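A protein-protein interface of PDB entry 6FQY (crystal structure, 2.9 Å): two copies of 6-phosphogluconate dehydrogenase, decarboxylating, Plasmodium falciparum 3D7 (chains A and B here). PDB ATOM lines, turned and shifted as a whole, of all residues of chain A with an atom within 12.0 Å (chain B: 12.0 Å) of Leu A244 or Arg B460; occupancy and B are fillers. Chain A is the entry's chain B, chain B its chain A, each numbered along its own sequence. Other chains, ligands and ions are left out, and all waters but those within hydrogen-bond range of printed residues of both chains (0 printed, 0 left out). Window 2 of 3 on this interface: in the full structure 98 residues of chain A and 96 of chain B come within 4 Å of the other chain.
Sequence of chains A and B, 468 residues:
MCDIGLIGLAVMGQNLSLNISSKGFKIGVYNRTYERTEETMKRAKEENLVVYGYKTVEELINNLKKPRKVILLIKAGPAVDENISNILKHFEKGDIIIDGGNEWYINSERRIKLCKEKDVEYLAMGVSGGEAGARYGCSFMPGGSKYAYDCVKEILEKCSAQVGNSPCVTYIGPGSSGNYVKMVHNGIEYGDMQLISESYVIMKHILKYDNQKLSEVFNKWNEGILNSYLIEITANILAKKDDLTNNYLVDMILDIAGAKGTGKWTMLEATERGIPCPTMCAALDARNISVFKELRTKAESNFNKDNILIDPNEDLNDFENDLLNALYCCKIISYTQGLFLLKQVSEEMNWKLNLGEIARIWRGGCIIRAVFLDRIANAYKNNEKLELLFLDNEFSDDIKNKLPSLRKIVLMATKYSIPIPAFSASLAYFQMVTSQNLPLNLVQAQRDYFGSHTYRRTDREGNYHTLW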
ATOM      1  N   LYS A 240     -12.245  17.550   6.497  1.00  0.00           N
ATOM      2  CA  LYS A 240     -13.342  18.499   6.369  1.00  0.00           C
ATOM      3  C   LYS A 240     -14.674  17.776   6.518  1.00  0.00           C
ATOM      4  O   LYS A 240     -14.883  16.708   5.934  1.00  0.00           O
ATOM      5  CB  LYS A 240     -13.270  19.216   5.022  1.00  0.00           C
ATOM      6  CG  LYS A 240     -14.266  20.354   4.877  1.00  0.00           C
ATOM      7  CD  LYS A 240     -13.777  21.589   5.620  1.00  0.00           C
ATOM      8  CE  LYS A 240     -14.866  22.644   5.737  1.00  0.00           C
ATOM      9  NZ  LYS A 240     -15.152  23.306   4.435  1.00  0.00           N
ATOM     10  N   LYS A 241     -15.577  18.360   7.297  1.00  0.00           N
ATOM     11  CA  LYS A 241     -16.885  17.775   7.550  1.00  0.00           C
ATOM     12  C   LYS A 241     -17.945  18.482   6.717  1.00  0.00           C
ATOM     13  O   LYS A 241     -17.885  19.699   6.519  1.00  0.00           O
ATOM     14  CB  LYS A 241     -17.244  17.858   9.035  1.00  0.00           C
ATOM     15  CG  LYS A 241     -16.129  17.419   9.971  1.00  0.00           C
ATOM     16  CD  LYS A 241     -16.675  16.619  11.143  1.00  0.00           C
ATOM     17  CE  LYS A 241     -15.695  16.599  12.306  1.00  0.00           C
ATOM     18  NZ  LYS A 241     -16.215  17.339  13.488  1.00  0.00           N
ATOM     19  N   ASP A 242     -18.910  17.711   6.225  1.00  0.00           N
ATOM     20  CA  ASP A 242     -20.014  18.294   5.483  1.00  0.00           C
ATOM     21  C   ASP A 242     -20.916  19.084   6.425  1.00  0.00           C
ATOM     22  O   ASP A 242     -21.075  18.747   7.600  1.00  0.00           O
ATOM     23  CB  ASP A 242     -20.815  17.197   4.778  1.00  0.00           C
ATOM     24  CG  ASP A 242     -21.743  17.741   3.710  1.00  0.00           C
ATOM     25  OD1 ASP A 242     -22.451  16.934   3.068  1.00  0.00           O
ATOM     26  OD2 ASP A 242     -21.769  18.973   3.507  1.00  0.00           O
ATOM     27  N   ASP A 243     -21.510  20.148   5.895  1.00  0.00           N
ATOM     28  CA  ASP A 243     -22.507  20.918   6.624  1.00  0.00           C
ATOM     29  C   ASP A 243     -23.914  20.635   6.135  1.00  0.00           C
ATOM     30  O   ASP A 243     -24.873  21.186   6.684  1.00  0.00           O
ATOM     31  CB  ASP A 243     -22.240  22.416   6.467  1.00  0.00           C
ATOM     32  CG  ASP A 243     -22.010  22.808   5.024  1.00  0.00           C
ATOM     33  OD1 ASP A 243     -21.630  21.927   4.223  1.00  0.00           O
ATOM     34  OD2 ASP A 243     -22.220  23.988   4.692  1.00  0.00           O
ATOM     35  N   LEU A 244     -24.053  19.776   5.135  1.00  0.00           N
ATOM     36  CA  LEU A 244     -25.352  19.390   4.612  1.00  0.00           C
ATOM     37  C   LEU A 244     -25.851  18.076   5.211  1.00  0.00           C
ATOM     38  O   LEU A 244     -27.057  17.924   5.436  1.00  0.00           O
ATOM     39  CB  LEU A 244     -25.260  19.271   3.086  1.00  0.00           C
ATOM     40  CG  LEU A 244     -25.066  20.569   2.287  1.00  0.00           C
ATOM     41  CD1 LEU A 244     -25.698  20.476   0.911  1.00  0.00           C
ATOM     42  CD2 LEU A 244     -25.561  21.808   3.027  1.00  0.00           C
ATOM     43  N   THR A 245     -24.952  17.128   5.487  1.00  0.00           N
ATOM     44  CA  THR A 245     -25.268  15.848   6.115  1.00  0.00           C
ATOM     45  C   THR A 245     -24.375  15.625   7.331  1.00  0.00           C
ATOM     46  O   THR A 245     -23.587  16.485   7.723  1.00  0.00           O
ATOM     47  CB  THR A 245     -25.123  14.688   5.119  1.00  0.00           C
ATOM     48  OG1 THR A 245     -23.733  14.388   4.947  1.00  0.00           O
ATOM     49  CG2 THR A 245     -25.742  15.047   3.771  1.00  0.00           C
ATOM     50  N   ASN A 246     -24.508  14.443   7.934  1.00  0.00           N
ATOM     51  CA  ASN A 246     -23.728  14.051   9.102  1.00  0.00           C
ATOM     52  C   ASN A 246     -22.407  13.378   8.731  1.00  0.00           C
ATOM     53  O   ASN A 246     -21.767  12.759   9.589  1.00  0.00           O
ATOM     54  CB  ASN A 246     -24.560  13.116   9.985  1.00  0.00           C
ATOM     55  CG  ASN A 246     -25.809  13.772  10.525  1.00  0.00           C
ATOM     56  OD1 ASN A 246     -26.931  13.303  10.269  1.00  0.00           O
ATOM     57  ND2 ASN A 246     -25.637  14.827  11.282  1.00  0.00           N
ATOM     58  N   ASN A 247     -21.975  13.496   7.481  1.00  0.00           N
ATOM     59  CA  ASN A 247     -20.795  12.788   7.013  1.00  0.00           C
ATOM     60  C   ASN A 247     -19.637  13.735   6.724  1.00  0.00           C
ATOM     61  O   ASN A 247     -19.779  14.959   6.739  1.00  0.00           O
ATOM     62  CB  ASN A 247     -21.151  11.961   5.779  1.00  0.00           C
ATOM     63  CG  ASN A 247     -22.287  11.000   6.052  1.00  0.00           C
ATOM     64  OD1 ASN A 247     -22.259  10.250   7.027  1.00  0.00           O
ATOM     65  ND2 ASN A 247     -23.301  11.024   5.195  1.00  0.00           N
ATOM     66  N   TYR A 248     -18.473  13.140   6.465  1.00  0.00           N
ATOM     67  CA  TYR A 248     -17.351  13.899   5.932  1.00  0.00           C
ATOM     68  C   TYR A 248     -17.653  14.323   4.502  1.00  0.00           C
ATOM     69  O   TYR A 248     -18.283  13.585   3.739  1.00  0.00           O
ATOM     70  CB  TYR A 248     -16.060  13.078   5.974  1.00  0.00           C
ATOM     71  CG  TYR A 248     -15.479  12.862   7.355  1.00  0.00           C
ATOM     72  CD1 TYR A 248     -15.766  11.716   8.083  1.00  0.00           C
ATOM     73  CD2 TYR A 248     -14.629  13.804   7.924  1.00  0.00           C
ATOM     74  CE1 TYR A 248     -15.233  11.518   9.345  1.00  0.00           C
ATOM     75  CE2 TYR A 248     -14.092  13.614   9.181  1.00  0.00           C
ATOM     76  CZ  TYR A 248     -14.396  12.470   9.887  1.00  0.00           C
ATOM     77  OH  TYR A 248     -13.859  12.284  11.140  1.00  0.00           O
ATOM     78  N   LEU A 249     -17.201  15.526   4.140  1.00  0.00           N
ATOM     79  CA  LEU A 249     -17.547  16.086   2.837  1.00  0.00           C
ATOM     80  C   LEU A 249     -17.008  15.229   1.697  1.00  0.00           C
ATOM     81  O   LEU A 249     -17.656  15.098   0.650  1.00  0.00           O
ATOM     82  CB  LEU A 249     -17.023  17.517   2.726  1.00  0.00           C
ATOM     83  CG  LEU A 249     -17.364  18.268   1.437  1.00  0.00           C
ATOM     84  CD1 LEU A 249     -18.858  18.217   1.167  1.00  0.00           C
ATOM     85  CD2 LEU A 249     -16.877  19.704   1.510  1.00  0.00           C
ATOM     86  N   VAL A 250     -15.823  14.640   1.877  1.00  0.00           N
ATOM     87  CA  VAL A 250     -15.223  13.839   0.811  1.00  0.00           C
ATOM     88  C   VAL A 250     -16.063  12.602   0.516  1.00  0.00           C
ATOM     89  O   VAL A 250     -16.065  12.103  -0.616  1.00  0.00           O
ATOM     90  CB  VAL A 250     -13.768  13.475   1.168  1.00  0.00           C
ATOM     91  CG1 VAL A 250     -13.716  12.300   2.128  1.00  0.00           C
ATOM     92  CG2 VAL A 250     -12.977  13.171  -0.094  1.00  0.00           C
ATOM     93  N   ASP A 251     -16.788  12.088   1.511  1.00  0.00           N
ATOM     94  CA  ASP A 251     -17.611  10.902   1.313  1.00  0.00           C
ATOM     95  C   ASP A 251     -18.915  11.196   0.584  1.00  0.00           C
ATOM     96  O   ASP A 251     -19.625  10.254   0.218  1.00  0.00           O
ATOM     97  CB  ASP A 251     -17.917  10.237   2.659  1.00  0.00           C
ATOM     98  CG  ASP A 251     -16.695   9.589   3.282  1.00  0.00           C
ATOM     99  OD1 ASP A 251     -15.803   9.150   2.526  1.00  0.00           O
ATOM    100  OD2 ASP A 251     -16.629   9.514   4.527  1.00  0.00           O
ATOM    101  N   MET A 252     -19.248  12.468   0.369  1.00  0.00           N
ATOM    102  CA  MET A 252     -20.461  12.849  -0.342  1.00  0.00           C
ATOM    103  C   MET A 252     -20.173  13.405  -1.730  1.00  0.00           C
ATOM    104  O   MET A 252     -21.100  13.861  -2.409  1.00  0.00           O
ATOM    105  CB  MET A 252     -21.261  13.863   0.479  1.00  0.00           C
ATOM    106  CG  MET A 252     -21.450  13.466   1.932  1.00  0.00           C
ATOM    107  SD  MET A 252     -22.632  12.117   2.118  1.00  0.00           S
ATOM    108  CE  MET A 252     -24.048  12.791   1.254  1.00  0.00           C
ATOM    109  N   ILE A 253     -18.918  13.385  -2.165  1.00  0.00           N
ATOM    110  CA  ILE A 253     -18.544  13.828  -3.503  1.00  0.00           C
ATOM    111  C   ILE A 253     -18.624  12.636  -4.444  1.00  0.00           C
ATOM    112  O   ILE A 253     -18.083  11.562  -4.149  1.00  0.00           O
ATOM    113  CB  ILE A 253     -17.135  14.446  -3.505  1.00  0.00           C
ATOM    114  CG1 ILE A 253     -17.071  15.618  -2.524  1.00  0.00           C
ATOM    115  CG2 ILE A 253     -16.754  14.901  -4.904  1.00  0.00           C
ATOM    116  CD1 ILE A 253     -15.696  16.220  -2.387  1.00  0.00           C
ATOM    117  N   LEU A 254     -19.290  12.820  -5.580  1.00  0.00           N
ATOM    118  CA  LEU A 254     -19.460  11.723  -6.520  1.00  0.00           C
ATOM    119  C   LEU A 254     -18.155  11.467  -7.263  1.00  0.00           C
ATOM    120  O   LEU A 254     -17.478  12.399  -7.704  1.00  0.00           O
ATOM    121  CB  LEU A 254     -20.589  12.042  -7.501  1.00  0.00           C
ATOM    122  CG  LEU A 254     -20.709  11.208  -8.775  1.00  0.00           C
ATOM    123  CD1 LEU A 254     -21.425   9.897  -8.486  1.00  0.00           C
ATOM    124  CD2 LEU A 254     -21.443  11.992  -9.847  1.00  0.00           C
ATOM    125  N   ASP A 255     -17.803  10.189  -7.399  1.00  0.00           N
ATOM    126  CA  ASP A 255     -16.477   9.792  -7.878  1.00  0.00           C
ATOM    127  C   ASP A 255     -16.429   9.754  -9.407  1.00  0.00           C
ATOM    128  O   ASP A 255     -16.216   8.716 -10.034  1.00  0.00           O
ATOM    129  CB  ASP A 255     -16.085   8.447  -7.276  1.00  0.00           C
ATOM    130  CG  ASP A 255     -17.123   7.373  -7.523  1.00  0.00           C
ATOM    131  OD1 ASP A 255     -18.329   7.701  -7.527  1.00  0.00           O
ATOM    132  OD2 ASP A 255     -16.734   6.202  -7.718  1.00  0.00           O
ATOM    133  N   ILE A 256     -16.629  10.924 -10.006  1.00  0.00           N
ATOM    134  CA  ILE A 256     -16.468  11.120 -11.443  1.00  0.00           C
ATOM    135  C   ILE A 256     -15.537  12.308 -11.636  1.00  0.00           C
ATOM    136  O   ILE A 256     -15.916  13.450 -11.353  1.00  0.00           O
ATOM    137  CB  ILE A 256     -17.803  11.353 -12.159  1.00  0.00           C
ATOM    138  CG1 ILE A 256     -18.709  10.135 -11.997  1.00  0.00           C
ATOM    139  CG2 ILE A 256     -17.568  11.648 -13.632  1.00  0.00           C
ATOM    140  CD1 ILE A 256     -19.947  10.203 -12.840  1.00  0.00           C
ATOM    141  N   LYS A 293     -19.704   5.663 -14.719  1.00  0.00           N
ATOM    142  CA  LYS A 293     -20.203   5.397 -13.374  1.00  0.00           C
ATOM    143  C   LYS A 293     -21.365   4.412 -13.399  1.00  0.00           C
ATOM    144  O   LYS A 293     -21.468   3.543 -12.525  1.00  0.00           O
ATOM    145  CB  LYS A 293     -20.621   6.710 -12.715  1.00  0.00           C
ATOM    146  CG  LYS A 293     -21.398   6.559 -11.420  1.00  0.00           C
ATOM    147  CD  LYS A 293     -20.508   6.052 -10.303  1.00  0.00           C
ATOM    148  CE  LYS A 293     -21.244   6.050  -8.976  1.00  0.00           C
ATOM    149  NZ  LYS A 293     -20.345   5.722  -7.835  1.00  0.00           N
ATOM    150  N   GLN B 444     -11.530  14.670  -7.150  1.00  0.00           N
ATOM    151  CA  GLN B 444     -12.443  15.784  -7.386  1.00  0.00           C
ATOM    152  C   GLN B 444     -12.369  16.799  -6.255  1.00  0.00           C
ATOM    153  O   GLN B 444     -12.478  18.009  -6.487  1.00  0.00           O
ATOM    154  CB  GLN B 444     -13.875  15.273  -7.548  1.00  0.00           C
ATOM    155  CG  GLN B 444     -14.194  14.746  -8.929  1.00  0.00           C
ATOM    156  CD  GLN B 444     -14.202  15.836  -9.982  1.00  0.00           C
ATOM    157  OE1 GLN B 444     -13.193  16.082 -10.646  1.00  0.00           O
ATOM    158  NE2 GLN B 444     -15.341  16.498 -10.141  1.00  0.00           N
ATOM    159  N   THR B 454     -14.963  22.799  -9.243  1.00  0.00           N
ATOM    160  CA  THR B 454     -16.266  22.364  -8.746  1.00  0.00           C
ATOM    161  C   THR B 454     -16.381  20.843  -8.732  1.00  0.00           C
ATOM    162  O   THR B 454     -15.623  20.139  -9.408  1.00  0.00           O
ATOM    163  CB  THR B 454     -17.414  22.981  -9.560  1.00  0.00           C
ATOM    164  OG1 THR B 454     -17.525  22.318 -10.825  1.00  0.00           O
ATOM    165  CG2 THR B 454     -17.189  24.474  -9.775  1.00  0.00           C
ATOM    166  N   TYR B 455     -17.326  20.327  -7.951  1.00  0.00           N
ATOM    167  CA  TYR B 455     -17.562  18.897  -7.845  1.00  0.00           C
ATOM    168  C   TYR B 455     -19.058  18.646  -7.751  1.00  0.00           C
ATOM    169  O   TYR B 455     -19.850  19.559  -7.506  1.00  0.00           O
ATOM    170  CB  TYR B 455     -16.823  18.296  -6.640  1.00  0.00           C
ATOM    171  CG  TYR B 455     -17.295  18.820  -5.304  1.00  0.00           C
ATOM    172  CD1 TYR B 455     -16.712  19.945  -4.737  1.00  0.00           C
ATOM    173  CD2 TYR B 455     -18.321  18.192  -4.606  1.00  0.00           C
ATOM    174  CE1 TYR B 455     -17.136  20.433  -3.519  1.00  0.00           C
ATOM    175  CE2 TYR B 455     -18.752  18.674  -3.384  1.00  0.00           C
ATOM    176  CZ  TYR B 455     -18.154  19.795  -2.845  1.00  0.00           C
ATOM    177  OH  TYR B 455     -18.574  20.284  -1.629  1.00  0.00           O
ATOM    178  N   ARG B 456     -19.444  17.392  -7.958  1.00  0.00           N
ATOM    179  CA  ARG B 456     -20.834  16.982  -7.856  1.00  0.00           C
ATOM    180  C   ARG B 456     -21.006  16.154  -6.588  1.00  0.00           C
ATOM    181  O   ARG B 456     -20.045  15.582  -6.066  1.00  0.00           O
ATOM    182  CB  ARG B 456     -21.246  16.170  -9.091  1.00  0.00           C
ATOM    183  CG  ARG B 456     -21.391  17.013 -10.357  1.00  0.00           C
ATOM    184  CD  ARG B 456     -22.620  16.675 -11.196  1.00  0.00           C
ATOM    185  NE  ARG B 456     -22.816  15.249 -11.443  1.00  0.00           N
ATOM    186  CZ  ARG B 456     -22.316  14.580 -12.479  1.00  0.00           C
ATOM    187  NH1 ARG B 456     -21.563  15.193 -13.383  1.00  0.00           N
ATOM    188  NH2 ARG B 456     -22.574  13.287 -12.606  1.00  0.00           N
ATOM    189  N   ARG B 457     -22.234  16.095  -6.081  1.00  0.00           N
ATOM    190  CA  ARG B 457     -22.481  15.407  -4.823  1.00  0.00           C
ATOM    191  C   ARG B 457     -23.288  14.134  -5.034  1.00  0.00           C
ATOM    192  O   ARG B 457     -23.996  13.965  -6.030  1.00  0.00           O
ATOM    193  CB  ARG B 457     -23.212  16.296  -3.808  1.00  0.00           C
ATOM    194  CG  ARG B 457     -22.501  17.575  -3.415  1.00  0.00           C
ATOM    195  CD  ARG B 457     -23.322  18.329  -2.378  1.00  0.00           C
ATOM    196  NE  ARG B 457     -23.741  17.448  -1.287  1.00  0.00           N
ATOM    197  CZ  ARG B 457     -23.453  17.640  -0.002  1.00  0.00           C
ATOM    198  NH1 ARG B 457     -22.739  18.691   0.375  1.00  0.00           N
ATOM    199  NH2 ARG B 457     -23.881  16.775   0.908  1.00  0.00           N
ATOM    200  N   THR B 458     -23.146  13.231  -4.061  1.00  0.00           N
ATOM    201  CA  THR B 458     -23.943  12.010  -4.019  1.00  0.00           C
ATOM    202  C   THR B 458     -25.436  12.320  -4.006  1.00  0.00           C
ATOM    203  O   THR B 458     -26.194  11.817  -4.843  1.00  0.00           O
ATOM    204  CB  THR B 458     -23.550  11.175  -2.799  1.00  0.00           C
ATOM    205  OG1 THR B 458     -22.159  10.844  -2.877  1.00  0.00           O
ATOM    206  CG2 THR B 458     -24.360   9.890  -2.752  1.00  0.00           C
ATOM    207  N   ASP B 459     -25.879  13.143  -3.057  1.00  0.00           N
ATOM    208  CA  ASP B 459     -27.281  13.192  -2.664  1.00  0.00           C
ATOM    209  C   ASP B 459     -28.069  14.316  -3.324  1.00  0.00           C
ATOM    210  O   ASP B 459     -29.252  14.483  -3.008  1.00  0.00           O
ATOM    211  CB  ASP B 459     -27.389  13.332  -1.142  1.00  0.00           C
ATOM    212  CG  ASP B 459     -26.602  14.516  -0.605  1.00  0.00           C
ATOM    213  OD1 ASP B 459     -26.776  14.859   0.585  1.00  0.00           O
ATOM    214  OD2 ASP B 459     -25.824  15.115  -1.377  1.00  0.00           O
ATOM    215  N   ARG B 460     -27.465  15.090  -4.221  1.00  0.00           N
ATOM    216  CA  ARG B 460     -28.180  16.224  -4.790  1.00  0.00           C
ATOM    217  C   ARG B 460     -27.559  16.557  -6.136  1.00  0.00           C
ATOM    218  O   ARG B 460     -26.419  16.182  -6.419  1.00  0.00           O
ATOM    219  CB  ARG B 460     -28.137  17.437  -3.859  1.00  0.00           C
ATOM    220  CG  ARG B 460     -26.786  17.674  -3.226  1.00  0.00           C
ATOM    221  CD  ARG B 460     -26.896  18.659  -2.090  1.00  0.00           C
ATOM    222  NE  ARG B 460     -27.510  17.977  -0.957  1.00  0.00           N
ATOM    223  CZ  ARG B 460     -28.330  18.532  -0.075  1.00  0.00           C
ATOM    224  NH1 ARG B 460     -28.681  19.807  -0.185  1.00  0.00           N
ATOM    225  NH2 ARG B 460     -28.809  17.796   0.914  1.00  0.00           N
ATOM    226  N   GLU B 461     -28.321  17.266  -6.961  1.00  0.00           N
ATOM    227  CA  GLU B 461     -27.807  17.721  -8.242  1.00  0.00           C
ATOM    228  C   GLU B 461     -27.109  19.071  -8.107  1.00  0.00           C
ATOM    229  O   GLU B 461     -27.112  19.706  -7.050  1.00  0.00           O
ATOM    230  CB  GLU B 461     -28.933  17.794  -9.273  1.00  0.00           C
ATOM    231  CG  GLU B 461     -29.657  16.479  -9.444  1.00  0.00           C
ATOM    232  CD  GLU B 461     -28.894  15.528 -10.342  1.00  0.00           C
ATOM    233  OE1 GLU B 461     -29.349  14.381 -10.527  1.00  0.00           O
ATOM    234  OE2 GLU B 461     -27.819  15.917 -10.845  1.00  0.00           O
ATOM    235  N   GLY B 462     -26.508  19.506  -9.209  1.00  0.00           N
ATOM    236  CA  GLY B 462     -25.788  20.759  -9.249  1.00  0.00           C
ATOM    237  C   GLY B 462     -24.300  20.582  -8.997  1.00  0.00           C
ATOM    238  O   GLY B 462     -23.837  19.568  -8.474  1.00  0.00           O
ATOM    239  N   ASN B 463     -23.541  21.601  -9.386  1.00  0.00           N
ATOM    240  CA  ASN B 463     -22.105  21.642  -9.159  1.00  0.00           C
ATOM    241  C   ASN B 463     -21.814  22.566  -7.984  1.00  0.00           C
ATOM    242  O   ASN B 463     -22.371  23.664  -7.895  1.00  0.00           O
ATOM    243  CB  ASN B 463     -21.369  22.123 -10.411  1.00  0.00           C
ATOM    244  CG  ASN B 463     -21.706  21.297 -11.641  1.00  0.00           C
ATOM    245  OD1 ASN B 463     -21.947  20.092 -11.548  1.00  0.00           O
ATOM    246  ND2 ASN B 463     -21.733  21.943 -12.800  1.00  0.00           N
ATOM    247  N   TYR B 464     -20.940  22.121  -7.084  1.00  0.00           N
ATOM    248  CA  TYR B 464     -20.695  22.832  -5.839  1.00  0.00           C
ATOM    249  C   TYR B 464     -19.210  23.123  -5.671  1.00  0.00           C
ATOM    250  O   TYR B 464     -18.354  22.393  -6.178  1.00  0.00           O
ATOM    251  CB  TYR B 464     -21.205  22.028  -4.633  1.00  0.00           C
ATOM    252  CG  TYR B 464     -22.684  21.714  -4.695  1.00  0.00           C
ATOM    253  CD1 TYR B 464     -23.150  20.603  -5.387  1.00  0.00           C
ATOM    254  CD2 TYR B 464     -23.616  22.533  -4.068  1.00  0.00           C
ATOM    255  CE1 TYR B 464     -24.499  20.314  -5.450  1.00  0.00           C
ATOM    256  CE2 TYR B 464     -24.968  22.252  -4.126  1.00  0.00           C
ATOM    257  CZ  TYR B 464     -25.404  21.141  -4.819  1.00  0.00           C
ATOM    258  OH  TYR B 464     -26.748  20.856  -4.879  1.00  0.00           O
ATOM    259  N   HIS B 465     -18.919  24.207  -4.952  1.00  0.00           N
ATOM    260  CA  HIS B 465     -17.560  24.582  -4.588  1.00  0.00           C
ATOM    261  C   HIS B 465     -17.526  24.982  -3.119  1.00  0.00           C
ATOM    262  O   HIS B 465     -18.433  25.664  -2.633  1.00  0.00           O
ATOM    263  CB  HIS B 465     -17.056  25.735  -5.464  1.00  0.00           C
ATOM    264  CG  HIS B 465     -15.788  26.359  -4.975  1.00  0.00           C
ATOM    265  ND1 HIS B 465     -14.596  25.671  -4.909  1.00  0.00           N
ATOM    266  CD2 HIS B 465     -15.526  27.609  -4.524  1.00  0.00           C
ATOM    267  CE1 HIS B 465     -13.654  26.470  -4.441  1.00  0.00           C
ATOM    268  NE2 HIS B 465     -14.193  27.652  -4.198  1.00  0.00           N
ATOM    269  N   THR B 466     -16.477  24.555  -2.414  1.00  0.00           N
ATOM    270  CA  THR B 466     -16.354  24.768  -0.978  1.00  0.00           C
ATOM    271  C   THR B 466     -14.986  25.340  -0.631  1.00  0.00           C
ATOM    272  O   THR B 466     -13.978  24.982  -1.247  1.00  0.00           O
ATOM    273  CB  THR B 466     -16.589  23.470  -0.199  1.00  0.00           C
ATOM    274  OG1 THR B 466     -16.166  23.641   1.160  1.00  0.00           O
ATOM    275  CG2 THR B 466     -15.817  22.330  -0.828  1.00  0.00           C
ATOM    276  N   LEU B 467     -14.965  26.237   0.354  1.00  0.00           N
ATOM    277  CA  LEU B 467     -13.728  26.727   0.964  1.00  0.00           C
ATOM    278  C   LEU B 467     -13.313  25.757   2.065  1.00  0.00           C
ATOM    279  O   LEU B 467     -13.882  25.757   3.158  1.00  0.00           O
ATOM    280  CB  LEU B 467     -13.920  28.140   1.506  1.00  0.00           C
ATOM    281  CG  LEU B 467     -12.879  28.679   2.494  1.00  0.00           C
ATOM    282  CD1 LEU B 467     -11.508  28.807   1.844  1.00  0.00           C
ATOM    283  CD2 LEU B 467     -13.328  30.011   3.078  1.00  0.00           C
ATOM    284  N   TRP B 468     -12.325  24.915   1.774  1.00  0.00           N
ATOM    285  CA  TRP B 468     -11.916  23.846   2.687  1.00  0.00           C
ATOM    286  C   TRP B 468     -11.159  24.358   3.913  1.00  0.00           C
ATOM    287  O   TRP B 468     -10.842  23.584   4.818  1.00  0.00           O
ATOM    288  CB  TRP B 468     -11.055  22.817   1.950  1.00  0.00           C
ATOM    289  CG  TRP B 468     -11.690  22.254   0.715  1.00  0.00           C
ATOM    290  CD1 TRP B 468     -11.747  22.830  -0.521  1.00  0.00           C
ATOM    291  CD2 TRP B 468     -12.347  20.987   0.599  1.00  0.00           C
ATOM    292  NE1 TRP B 468     -12.407  22.002  -1.397  1.00  0.00           N
ATOM    293  CE2 TRP B 468     -12.783  20.863  -0.735  1.00  0.00           C
ATOM    294  CE3 TRP B 468     -12.611  19.946   1.494  1.00  0.00           C
ATOM    295  CZ2 TRP B 468     -13.471  19.741  -1.193  1.00  0.00           C
ATOM    296  CZ3 TRP B 468     -13.292  18.834   1.037  1.00  0.00           C
ATOM    297  CH2 TRP B 468     -13.714  18.740  -0.294  1.00  0.00           C
ATOM    298  OXT TRP B 468     -10.828  25.536   4.034  1.00  0.00           O
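No position is printed for both chains.
Of the 21 pairs that touch across the chains among the printed residues, none has its exchanged pair printed and touching as well.
The backbone carbonyl oxygen (O) of Tyr B455 lies within hydrogen-bond range of the backbone NH (N) of Tyr B464 (2.8 Å).
NE of Arg B457 lies within salt-bridge range of OD2 of Asp B459, 3.1 Å away.
The backbone carbonyl oxygen (O) of Thr B466 sits close to the indole nitrogen (NE1) of Trp B468, 3.4 Å away.
The backbone carbonyl oxygen (O) of Lys A240 is in hydrogen-bond range of the backbone NH (N) of Leu A249 (3.2 Å).
The side-chain sulfur of Met A252 sits at hydrogen-bond distance from the side-chain amide nitrogen of Asn A247, 3.3 Å away.
Asp A242 touches just one residue of chain B: Arg B457.
Leu A244 touches just these residues of chain B: Arg B457 and Arg B460.
Of the printed residues of chain B, Leu A254 touches Arg B456.
Of the printed residues of chain A, Tyr B455 touches Leu A249 (3.5 Å) and Ile A253 (3.5 Å).
Of chain A, only Met A252 (2.7 Å) comes within 4 Å of Thr B458.
Asp B459 touches two residues of chain A.
Arg B460 touches one residue of chain A.
No residue of chain A comes within 4 Å of Glu B461.
No residue of chain A comes within 4 Å of Gly B462.
His B465 touches none of the printed residues of chain A.
The nearest residue of chain B that does not touch Leu A244 is Asp B459 (5.3 Å).
The nearest printed residue of chain B that does not touch Ile A253 is Thr B458 (4.2 Å).
Of the 16 printed residues of chain B, 10 touch a printed residue of chain A.
Hydrophobic or aromatic side chains of chain B that line the printed part of chain A: Tyr B455 and Trp B468.
Among the printed residues, Asp or Glu carboxylates within 4 Å of a Lys or Arg side-chain nitrogen of the other chain: Asp A242 with Arg B457.
The side-chain amide nitrogen (NE2) of Gln B444 lies close to the backbone carbonyl oxygen (O) of Ile A256 (3.3 Å).
The backbone carbonyl oxygen (O) of Arg B456 is in hydrogen-bond range of the backbone NH (N) of Leu A254, at 2.9 Å.
NH2 of Arg B457 lies within salt-bridge range of OD1 of Asp A242 (2.6 Å).
The backbone carbonyl oxygen (O) of Met A252 is in hydrogen-bond range of the backbone NH (N) of Thr B458, 2.7 Å away.
NZ of Lys A240 is in hydrogen-bond range of OG1 of Thr B466 (3.4 Å).
NZ of Lys A240 lies within hydrogen-bond range of O of Leu B467 (3.0 Å).
Among the printed residues, merely in contact across the chains: Met A252 with Arg B457 (3.2 Å), Leu A244 with Arg B460 (3.2 Å), Thr A245 with Asp B459 (3.4 Å), Ile A253 with Arg B456 (3.4 Å), Met A252 with Asp B459 (3.5 Å), Leu A249 with Tyr B455 (3.5 Å), Leu A244 with Arg B457 (3.5 Å), Ile A253 with Tyr B455 (3.5 Å), Lys A240 with Trp B468 (3.6 Å), Leu A249 with Thr B466 (3.7 Å), Leu A249 with Trp B468 (3.7 Å), Thr A245 with Arg B457 (3.8 Å), Ile A253 with Trp B468 (3.8 Å), Ile A253 with Gln B444 (3.9 Å) and Leu A249 with Arg B457 (3.99 Å).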
